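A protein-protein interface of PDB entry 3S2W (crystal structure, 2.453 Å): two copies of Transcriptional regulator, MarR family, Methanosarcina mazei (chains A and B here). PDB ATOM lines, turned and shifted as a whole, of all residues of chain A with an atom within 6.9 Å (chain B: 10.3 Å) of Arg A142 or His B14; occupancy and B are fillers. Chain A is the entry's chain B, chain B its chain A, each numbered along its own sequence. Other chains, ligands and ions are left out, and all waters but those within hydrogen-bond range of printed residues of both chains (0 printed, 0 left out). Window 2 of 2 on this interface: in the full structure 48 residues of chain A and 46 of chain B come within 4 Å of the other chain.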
ATOM      1  N   PHE A 133      25.305 -13.936   8.614  1.00  0.00           N
ATOM      2  CA  PHE A 133      23.902 -13.901   9.028  1.00  0.00           C
ATOM      3  C   PHE A 133      23.631 -14.536  10.373  1.00  0.00           C
ATOM      4  O   PHE A 133      22.486 -14.567  10.798  1.00  0.00           O
ATOM      5  CB  PHE A 133      23.008 -14.607   8.026  1.00  0.00           C
ATOM      6  CG  PHE A 133      22.637 -13.773   6.861  1.00  0.00           C
ATOM      7  CD1 PHE A 133      22.940 -12.436   6.832  1.00  0.00           C
ATOM      8  CD2 PHE A 133      21.981 -14.330   5.785  1.00  0.00           C
ATOM      9  CE1 PHE A 133      22.591 -11.668   5.746  1.00  0.00           C
ATOM     10  CE2 PHE A 133      21.630 -13.571   4.708  1.00  0.00           C
ATOM     11  CZ  PHE A 133      21.932 -12.241   4.684  1.00  0.00           C
ATOM     12  N   ASP A 137      17.366 -13.069  12.732  1.00  0.00           N
ATOM     13  CA  ASP A 137      16.186 -13.927  12.588  1.00  0.00           C
ATOM     14  C   ASP A 137      15.866 -14.072  11.097  1.00  0.00           C
ATOM     15  O   ASP A 137      16.489 -13.411  10.260  1.00  0.00           O
ATOM     16  CB  ASP A 137      14.977 -13.433  13.423  1.00  0.00           C
ATOM     17  CG  ASP A 137      14.503 -12.015  13.048  1.00  0.00           C
ATOM     18  OD1 ASP A 137      13.937 -11.327  13.928  1.00  0.00           O
ATOM     19  OD2 ASP A 137      14.666 -11.585  11.889  1.00  0.00           O
ATOM     20  N   ASP A 138      14.917 -14.936  10.759  1.00  0.00           N
ATOM     21  CA  ASP A 138      14.572 -15.150   9.357  1.00  0.00           C
ATOM     22  C   ASP A 138      14.170 -13.865   8.624  1.00  0.00           C
ATOM     23  O   ASP A 138      14.591 -13.645   7.487  1.00  0.00           O
ATOM     24  CB  ASP A 138      13.495 -16.227   9.218  1.00  0.00           C
ATOM     25  CG  ASP A 138      14.035 -17.629   9.477  1.00  0.00           C
ATOM     26  OD1 ASP A 138      15.261 -17.826   9.310  1.00  0.00           O
ATOM     27  OD2 ASP A 138      13.242 -18.529   9.846  1.00  0.00           O
ATOM     28  N   ARG A 139      13.385 -13.008   9.275  1.00  0.00           N
ATOM     29  CA  ARG A 139      12.886 -11.785   8.633  1.00  0.00           C
ATOM     30  C   ARG A 139      13.973 -10.728   8.380  1.00  0.00           C
ATOM     31  O   ARG A 139      13.899  -9.968   7.408  1.00  0.00           O
ATOM     32  CB  ARG A 139      11.727 -11.168   9.439  1.00  0.00           C
ATOM     33  CG  ARG A 139      11.267  -9.796   8.922  1.00  0.00           C
ATOM     34  CD  ARG A 139      10.911  -8.853  10.066  1.00  0.00           C
ATOM     35  NE  ARG A 139      10.728  -7.470   9.620  1.00  0.00           N
ATOM     36  CZ  ARG A 139      10.527  -6.439  10.440  1.00  0.00           C
ATOM     37  NH1 ARG A 139      10.483  -6.633  11.753  1.00  0.00           N
ATOM     38  NH2 ARG A 139      10.367  -5.213   9.948  1.00  0.00           N
ATOM     39  N   GLN A 140      14.969 -10.662   9.259  1.00  0.00           N
ATOM     40  CA  GLN A 140      16.060  -9.728   9.044  1.00  0.00           C
ATOM     41  C   GLN A 140      16.899 -10.236   7.872  1.00  0.00           C
ATOM     42  O   GLN A 140      17.346  -9.445   7.047  1.00  0.00           O
ATOM     43  CB  GLN A 140      16.911  -9.566  10.308  1.00  0.00           C
ATOM     44  CG  GLN A 140      16.171  -8.980  11.514  1.00  0.00           C
ATOM     45  CD  GLN A 140      16.969  -9.090  12.814  1.00  0.00           C
ATOM     46  OE1 GLN A 140      17.062 -10.167  13.412  1.00  0.00           O
ATOM     47  NE2 GLN A 140      17.555  -7.973  13.250  1.00  0.00           N
ATOM     48  N   ARG A 141      17.095 -11.557   7.787  1.00  0.00           N
ATOM     49  CA  ARG A 141      17.847 -12.139   6.676  1.00  0.00           C
ATOM     50  C   ARG A 141      17.206 -11.817   5.322  1.00  0.00           C
ATOM     51  O   ARG A 141      17.896 -11.471   4.369  1.00  0.00           O
ATOM     52  CB  ARG A 141      17.995 -13.648   6.814  1.00  0.00           C
ATOM     53  CG  ARG A 141      18.778 -14.119   8.009  1.00  0.00           C
ATOM     54  CD  ARG A 141      18.988 -15.639   7.955  1.00  0.00           C
ATOM     55  NE  ARG A 141      20.049 -16.085   8.859  1.00  0.00           N
ATOM     56  CZ  ARG A 141      19.855 -16.614  10.066  1.00  0.00           C
ATOM     57  NH1 ARG A 141      18.621 -16.786  10.527  1.00  0.00           N
ATOM     58  NH2 ARG A 141      20.895 -16.979  10.810  1.00  0.00           N
ATOM     59  N   ARG A 142      15.885 -11.925   5.244  1.00  0.00           N
ATOM     60  CA  ARG A 142      15.190 -11.695   3.989  1.00  0.00           C
ATOM     61  C   ARG A 142      15.246 -10.219   3.576  1.00  0.00           C
ATOM     62  O   ARG A 142      15.485  -9.901   2.409  1.00  0.00           O
ATOM     63  CB  ARG A 142      13.744 -12.197   4.078  1.00  0.00           C
ATOM     64  CG  ARG A 142      12.818 -11.628   3.011  1.00  0.00           C
ATOM     65  CD  ARG A 142      11.347 -11.931   3.296  1.00  0.00           C
ATOM     66  NE  ARG A 142      10.457 -10.958   2.662  1.00  0.00           N
ATOM     67  CZ  ARG A 142       9.951 -11.084   1.438  1.00  0.00           C
ATOM     68  NH1 ARG A 142       9.154 -10.141   0.954  1.00  0.00           N
ATOM     69  NH2 ARG A 142      10.238 -12.151   0.698  1.00  0.00           N
ATOM     70  N   GLU A 143      15.034  -9.315   4.527  1.00  0.00           N
ATOM     71  CA  GLU A 143      15.103  -7.892   4.211  1.00  0.00           C
ATOM     72  C   GLU A 143      16.521  -7.487   3.752  1.00  0.00           C
ATOM     73  O   GLU A 143      16.694  -6.685   2.832  1.00  0.00           O
ATOM     74  CB  GLU A 143      14.636  -7.051   5.403  1.00  0.00           C
ATOM     75  CG  GLU A 143      13.192  -7.333   5.817  1.00  0.00           C
ATOM     76  CD  GLU A 143      12.636  -6.303   6.804  1.00  0.00           C
ATOM     77  OE1 GLU A 143      11.390  -6.184   6.915  1.00  0.00           O
ATOM     78  OE2 GLU A 143      13.441  -5.618   7.475  1.00  0.00           O
ATOM     79  N   ILE A 144      17.526  -8.072   4.394  1.00  0.00           N
ATOM     80  CA  ILE A 144      18.917  -7.800   4.083  1.00  0.00           C
ATOM     81  C   ILE A 144      19.268  -8.248   2.667  1.00  0.00           C
ATOM     82  O   ILE A 144      19.892  -7.511   1.894  1.00  0.00           O
ATOM     83  CB  ILE A 144      19.822  -8.529   5.078  1.00  0.00           C
ATOM     84  CG1 ILE A 144      20.130  -7.614   6.236  1.00  0.00           C
ATOM     85  CG2 ILE A 144      21.133  -8.879   4.444  1.00  0.00           C
ATOM     86  CD1 ILE A 144      20.834  -6.393   5.747  1.00  0.00           C
ATOM     87  N   THR A 145      18.861  -9.466   2.335  1.00  0.00           N
ATOM     88  CA  THR A 145      19.127 -10.028   1.022  1.00  0.00           C
ATOM     89  C   THR A 145      18.438  -9.178  -0.019  1.00  0.00           C
ATOM     90  O   THR A 145      19.047  -8.779  -1.012  1.00  0.00           O
ATOM     91  CB  THR A 145      18.641 -11.481   0.936  1.00  0.00           C
ATOM     92  OG1 THR A 145      19.251 -12.221   1.994  1.00  0.00           O
ATOM     93  CG2 THR A 145      19.038 -12.114  -0.389  1.00  0.00           C
ATOM     94  N   ASN A 146      17.173  -8.871   0.228  1.00  0.00           N
ATOM     95  CA  ASN A 146      16.414  -8.092  -0.732  1.00  0.00           C
ATOM     96  C   ASN A 146      17.123  -6.781  -0.994  1.00  0.00           C
ATOM     97  O   ASN A 146      17.313  -6.372  -2.147  1.00  0.00           O
ATOM     98  CB  ASN A 146      15.004  -7.841  -0.231  1.00  0.00           C
ATOM     99  CG  ASN A 146      14.125  -7.242  -1.295  1.00  0.00           C
ATOM    100  OD1 ASN A 146      14.545  -7.101  -2.446  1.00  0.00           O
ATOM    101  ND2 ASN A 146      12.888  -6.896  -0.932  1.00  0.00           N
ATOM    102  N   SER A 147      17.544  -6.141   0.089  1.00  0.00           N
ATOM    103  CA  SER A 147      18.242  -4.870   0.002  1.00  0.00           C
ATOM    104  C   SER A 147      19.553  -4.977  -0.789  1.00  0.00           C
ATOM    105  O   SER A 147      19.827  -4.142  -1.668  1.00  0.00           O
ATOM    106  CB  SER A 147      18.487  -4.307   1.403  1.00  0.00           C
ATOM    107  OG  SER A 147      17.252  -4.061   2.055  1.00  0.00           O
ATOM    108  N   LEU A 148      20.349  -6.004  -0.489  1.00  0.00           N
ATOM    109  CA  LEU A 148      21.598  -6.231  -1.228  1.00  0.00           C
ATOM    110  C   LEU A 148      21.381  -6.381  -2.729  1.00  0.00           C
ATOM    111  O   LEU A 148      22.140  -5.834  -3.498  1.00  0.00           O
ATOM    112  CB  LEU A 148      22.343  -7.448  -0.700  1.00  0.00           C
ATOM    113  CG  LEU A 148      23.000  -7.253   0.658  1.00  0.00           C
ATOM    114  CD1 LEU A 148      23.585  -8.580   1.138  1.00  0.00           C
ATOM    115  CD2 LEU A 148      24.053  -6.158   0.579  1.00  0.00           C
ATOM    116  N   GLU A 149      20.358  -7.139  -3.131  1.00  0.00           N
ATOM    117  CA  GLU A 149      20.019  -7.283  -4.538  1.00  0.00           C
ATOM    118  C   GLU A 149      19.753  -5.920  -5.161  1.00  0.00           C
ATOM    119  O   GLU A 149      20.221  -5.630  -6.256  1.00  0.00           O
ATOM    120  CB  GLU A 149      18.785  -8.169  -4.727  1.00  0.00           C
ATOM    121  CG  GLU A 149      19.046  -9.651  -4.501  1.00  0.00           C
ATOM    122  CD  GLU A 149      17.803 -10.533  -4.695  1.00  0.00           C
ATOM    123  OE1 GLU A 149      17.781 -11.661  -4.155  1.00  0.00           O
ATOM    124  OE2 GLU A 149      16.853 -10.107  -5.390  1.00  0.00           O
ATOM    125  N   GLY B  11      12.880 -17.232  -7.942  1.00  0.00           N
ATOM    126  CA  GLY B  11      11.739 -16.332  -7.933  1.00  0.00           C
ATOM    127  C   GLY B  11      10.620 -16.873  -7.064  1.00  0.00           C
ATOM    128  O   GLY B  11      10.129 -16.185  -6.174  1.00  0.00           O
ATOM    129  N   ILE B  12      10.204 -18.106  -7.338  1.00  0.00           N
ATOM    130  CA  ILE B  12       9.352 -18.837  -6.417  1.00  0.00           C
ATOM    131  C   ILE B  12      10.214 -19.322  -5.252  1.00  0.00           C
ATOM    132  O   ILE B  12       9.740 -19.435  -4.117  1.00  0.00           O
ATOM    133  CB  ILE B  12       8.686 -20.031  -7.092  1.00  0.00           C
ATOM    134  CG1 ILE B  12       7.277 -19.672  -7.542  1.00  0.00           C
ATOM    135  CG2 ILE B  12       8.522 -21.146  -6.112  1.00  0.00           C
ATOM    136  CD1 ILE B  12       6.281 -19.668  -6.407  1.00  0.00           C
ATOM    137  N   SER B  13      11.490 -19.592  -5.543  1.00  0.00           N
ATOM    138  CA  SER B  13      12.451 -20.038  -4.529  1.00  0.00           C
ATOM    139  C   SER B  13      12.678 -18.979  -3.454  1.00  0.00           C
ATOM    140  O   SER B  13      12.733 -19.295  -2.267  1.00  0.00           O
ATOM    141  CB  SER B  13      13.788 -20.452  -5.168  1.00  0.00           C
ATOM    142  OG  SER B  13      13.748 -21.788  -5.660  1.00  0.00           O
ATOM    143  N   HIS B  14      12.796 -17.723  -3.878  1.00  0.00           N
ATOM    144  CA  HIS B  14      12.996 -16.604  -2.955  1.00  0.00           C
ATOM    145  C   HIS B  14      11.719 -16.207  -2.187  1.00  0.00           C
ATOM    146  O   HIS B  14      11.780 -15.854  -1.010  1.00  0.00           O
ATOM    147  CB  HIS B  14      13.595 -15.401  -3.694  1.00  0.00           C
ATOM    148  CG  HIS B  14      12.965 -14.090  -3.332  1.00  0.00           C
ATOM    149  ND1 HIS B  14      11.652 -13.783  -3.637  1.00  0.00           N
ATOM    150  CD2 HIS B  14      13.464 -13.002  -2.700  1.00  0.00           C
ATOM    151  CE1 HIS B  14      11.372 -12.569  -3.201  1.00  0.00           C
ATOM    152  NE2 HIS B  14      12.453 -12.072  -2.629  1.00  0.00           N
ATOM    153  N   ALA B  15      10.567 -16.246  -2.847  1.00  0.00           N
ATOM    154  CA  ALA B  15       9.299 -15.959  -2.175  1.00  0.00           C
ATOM    155  C   ALA B  15       8.945 -17.062  -1.164  1.00  0.00           C
ATOM    156  O   ALA B  15       8.292 -16.814  -0.143  1.00  0.00           O
ATOM    157  CB  ALA B  15       8.182 -15.793  -3.198  1.00  0.00           C
ATOM    158  N   GLU B  16       9.393 -18.277  -1.469  1.00  0.00           N
ATOM    159  CA  GLU B  16       9.209 -19.444  -0.618  1.00  0.00           C
ATOM    160  C   GLU B  16      10.221 -19.449   0.524  1.00  0.00           C
ATOM    161  O   GLU B  16      10.151 -20.273   1.435  1.00  0.00           O
ATOM    162  CB  GLU B  16       9.390 -20.696  -1.463  1.00  0.00           C
ATOM    163  CG  GLU B  16       9.332 -21.992  -0.707  1.00  0.00           C
ATOM    164  CD  GLU B  16       9.330 -23.176  -1.645  1.00  0.00           C
ATOM    165  OE1 GLU B  16       8.395 -23.999  -1.560  1.00  0.00           O
ATOM    166  OE2 GLU B  16      10.256 -23.271  -2.478  1.00  0.00           O
ATOM    167  N   GLY B  17      11.172 -18.526   0.459  1.00  0.00           N
ATOM    168  CA  GLY B  17      12.145 -18.361   1.522  1.00  0.00           C
ATOM    169  C   GLY B  17      13.525 -18.878   1.189  1.00  0.00           C
ATOM    170  O   GLY B  17      14.510 -18.337   1.652  1.00  0.00           O
ATOM    171  N   LEU B  18      13.603 -19.937   0.393  1.00  0.00           N
ATOM    172  CA  LEU B  18      14.897 -20.499   0.031  1.00  0.00           C
ATOM    173  C   LEU B  18      15.804 -19.415  -0.528  1.00  0.00           C
ATOM    174  O   LEU B  18      15.335 -18.451  -1.131  1.00  0.00           O
ATOM    175  CB  LEU B  18      14.735 -21.644  -0.970  1.00  0.00           C
ATOM    176  CG  LEU B  18      14.065 -22.892  -0.394  1.00  0.00           C
ATOM    177  CD1 LEU B  18      14.459 -23.110   1.077  1.00  0.00           C
ATOM    178  CD2 LEU B  18      12.561 -22.828  -0.549  1.00  0.00           C
ATOM    179  N   CYS B  19      17.104 -19.558  -0.322  1.00  0.00           N
ATOM    180  CA  CYS B  19      18.026 -18.531  -0.787  1.00  0.00           C
ATOM    181  C   CYS B  19      19.338 -19.108  -1.304  1.00  0.00           C
ATOM    182  O   CYS B  19      19.743 -20.211  -0.929  1.00  0.00           O
ATOM    183  CB  CYS B  19      18.292 -17.503   0.324  1.00  0.00           C
ATOM    184  SG  CYS B  19      19.264 -16.052  -0.186  1.00  0.00           S
ATOM    185  N   ASP B  20      19.981 -18.354  -2.188  1.00  0.00           N
ATOM    186  CA  ASP B  20      21.356 -18.622  -2.580  1.00  0.00           C
ATOM    187  C   ASP B  20      22.243 -18.244  -1.380  1.00  0.00           C
ATOM    188  O   ASP B  20      22.475 -17.062  -1.111  1.00  0.00           O
ATOM    189  CB  ASP B  20      21.707 -17.797  -3.831  1.00  0.00           C
ATOM    190  CG  ASP B  20      22.903 -18.352  -4.602  1.00  0.00           C
ATOM    191  OD1 ASP B  20      23.110 -19.586  -4.593  1.00  0.00           O
ATOM    192  OD2 ASP B  20      23.631 -17.548  -5.230  1.00  0.00           O
ATOM    193  N   PHE B  23      24.873 -15.908  -2.065  1.00  0.00           N
ATOM    194  CA  PHE B  23      24.544 -14.611  -2.633  1.00  0.00           C
ATOM    195  C   PHE B  23      25.094 -13.418  -1.831  1.00  0.00           C
ATOM    196  O   PHE B  23      25.529 -12.426  -2.411  1.00  0.00           O
ATOM    197  CB  PHE B  23      23.037 -14.460  -2.857  1.00  0.00           C
ATOM    198  CG  PHE B  23      22.634 -13.066  -3.198  1.00  0.00           C
ATOM    199  CD1 PHE B  23      22.728 -12.606  -4.503  1.00  0.00           C
ATOM    200  CD2 PHE B  23      22.206 -12.193  -2.206  1.00  0.00           C
ATOM    201  CE1 PHE B  23      22.381 -11.305  -4.817  1.00  0.00           C
ATOM    202  CE2 PHE B  23      21.856 -10.895  -2.514  1.00  0.00           C
ATOM    203  CZ  PHE B  23      21.942 -10.451  -3.820  1.00  0.00           C
ATOM    204  N   ILE B  24      25.059 -13.533  -0.509  1.00  0.00           N
ATOM    205  CA  ILE B  24      25.584 -12.520   0.381  1.00  0.00           C
ATOM    206  C   ILE B  24      27.027 -12.171  -0.018  1.00  0.00           C
ATOM    207  O   ILE B  24      27.332 -11.025  -0.364  1.00  0.00           O
ATOM    208  CB  ILE B  24      25.553 -12.984   1.862  1.00  0.00           C
ATOM    209  CG1 ILE B  24      24.147 -13.412   2.288  1.00  0.00           C
ATOM    210  CG2 ILE B  24      26.007 -11.867   2.761  1.00  0.00           C
ATOM    211  CD1 ILE B  24      23.762 -14.864   1.926  1.00  0.00           C
ATOM    212  N   PHE B 136      15.682   3.637  -1.664  1.00  0.00           N
ATOM    213  CA  PHE B 136      15.493   3.469  -0.218  1.00  0.00           C
ATOM    214  C   PHE B 136      15.140   4.772   0.500  1.00  0.00           C
ATOM    215  O   PHE B 136      15.755   5.810   0.248  1.00  0.00           O
ATOM    216  CB  PHE B 136      16.741   2.870   0.429  1.00  0.00           C
ATOM    217  CG  PHE B 136      17.086   1.512  -0.092  1.00  0.00           C
ATOM    218  CD1 PHE B 136      16.242   0.431   0.145  1.00  0.00           C
ATOM    219  CD2 PHE B 136      18.236   1.312  -0.835  1.00  0.00           C
ATOM    220  CE1 PHE B 136      16.548  -0.823  -0.335  1.00  0.00           C
ATOM    221  CE2 PHE B 136      18.548   0.058  -1.317  1.00  0.00           C
ATOM    222  CZ  PHE B 136      17.709  -1.012  -1.063  1.00  0.00           C
ATOM    223  N   GLU B 143      18.222   0.807   8.520  1.00  0.00           N
ATOM    224  CA  GLU B 143      18.307  -0.551   9.030  1.00  0.00           C
ATOM    225  C   GLU B 143      19.218  -1.468   8.208  1.00  0.00           C
ATOM    226  O   GLU B 143      19.673  -2.508   8.696  1.00  0.00           O
ATOM    227  CB  GLU B 143      16.915  -1.165   9.229  1.00  0.00           C
ATOM    228  CG  GLU B 143      16.157  -1.457   7.971  1.00  0.00           C
ATOM    229  CD  GLU B 143      14.939  -2.320   8.241  1.00  0.00           C
ATOM    230  OE1 GLU B 143      14.970  -3.512   7.859  1.00  0.00           O
ATOM    231  OE2 GLU B 143      13.961  -1.813   8.844  1.00  0.00           O
ATOM    232  N   ILE B 144      19.487  -1.079   6.967  1.00  0.00           N
ATOM    233  CA  ILE B 144      20.450  -1.795   6.152  1.00  0.00           C
ATOM    234  C   ILE B 144      21.872  -1.432   6.592  1.00  0.00           C
ATOM    235  O   ILE B 144      22.771  -2.272   6.563  1.00  0.00           O
ATOM    236  CB  ILE B 144      20.240  -1.547   4.629  1.00  0.00           C
ATOM    237  CG1 ILE B 144      21.383  -2.152   3.831  1.00  0.00           C
ATOM    238  CG2 ILE B 144      20.153  -0.083   4.309  1.00  0.00           C
ATOM    239  CD1 ILE B 144      21.275  -3.681   3.697  1.00  0.00           C
ATOM    240  N   SER B 147      22.293  -3.313   9.670  1.00  0.00           N
ATOM    241  CA  SER B 147      22.489  -4.755   9.477  1.00  0.00           C
ATOM    242  C   SER B 147      23.904  -5.026   8.984  1.00  0.00           C
ATOM    243  O   SER B 147      24.519  -6.025   9.362  1.00  0.00           O
ATOM    244  CB  SER B 147      21.472  -5.358   8.500  1.00  0.00           C
ATOM    245  OG  SER B 147      20.127  -5.140   8.881  1.00  0.00           O
ATOM    246  N   MET B 151      26.695  -7.432  10.672  1.00  0.00           N
ATOM    247  CA  MET B 151      27.280  -8.479   9.859  1.00  0.00           C
ATOM    248  C   MET B 151      28.764  -8.434  10.008  1.00  0.00           C
ATOM    249  O   MET B 151      29.407  -9.470  10.083  1.00  0.00           O
ATOM    250  CB  MET B 151      26.889  -8.323   8.392  1.00  0.00           C
ATOM    251  CG  MET B 151      25.483  -8.785   8.141  1.00  0.00           C
ATOM    252  SD  MET B 151      24.893  -8.331   6.378  1.00  0.00           S
ATOM    253  CE  MET B 151      26.289  -9.189   5.335  1.00  0.00           C
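OE2 of Glu A143 lies close to OE1 of Glu B143 (2.6 Å).
The backbone carbonyl oxygen (O) of Glu B143 sits at hydrogen-bond distance from the side-chain hydroxyl (OG) of Ser B147.
The guanidinium group (NH2) of Arg A141 is in hydrogen-bond range of the backbone carbonyl oxygen (O) of Phe A133 (2.9 Å).
NE of Arg A139 is in salt-bridge range of OE1 of Glu A143, at 3.1 Å.
The side-chain hydroxyl of Thr A145 is in hydrogen-bond range of the backbone carbonyl oxygen of Arg A141, at 2.8 Å.
The side-chain hydroxyl (OG) of Ser A147 is in hydrogen-bond range of the backbone carbonyl oxygen (O) of Glu A143, 2.8 Å away.
Among the printed residues, pairs that only touch across the chains: Ile A144 with Ser B147, Glu A149 with Phe B23, Ile A144 with Ile B144, Phe A133 with Ile B24, Thr A145 with Phe B23, Ser A147 with Ile B144, Ser A147 with Phe B136, Leu A148 with Phe B23, Thr A145 with Cys B19 and Arg A142 with His B14.
Of the printed residues of chain B, Arg A142 touches His B14.
Of the printed residues of chain A, His B14 touches Arg A142 (3.998 Å).
Printed residues of chain B within 4 Å of Glu A143: Glu B143.
Printed residues of chain B within 4 Å of Ser A147: Phe B136 (3.8 Å) and Ile B144 (3.7 Å).
Of the printed residues of chain B, Glu A149 touches Phe B23 (3.1 Å).
Of the printed residues of chain A, Glu B143 touches Glu A143.
Gly B11 touches none of the printed residues of chain A.
Met B151 touches none of the printed residues of chain A.
The nearest printed residue of chain B that does not touch Ile A144 is Met B151 (4.3 Å).
Hydrophobic or aromatic side chains of chain B that line the printed part of chain A: His B14, Phe B23, Ile B24, Phe B136 and Ile B144.
Along chain B the printed residues that touch a printed residue of chain A span positions 14 to 147.
Of the 14 printed residues of chain A, 8 touch a printed residue of chain B.
Printed residues of chain A that touch a printed residue of chain B: Phe A133, Arg A142, Glu A143, Ile A144, Thr A145, Ser A147, Leu A148 and Glu A149.
Glu A143 touches its own counterpart, Glu B143.
Ile B144 touches its own counterpart, Ile A144.
Ile A144 touches Ser B147, and with the chains exchanged Ser A147 touches Ile B144.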
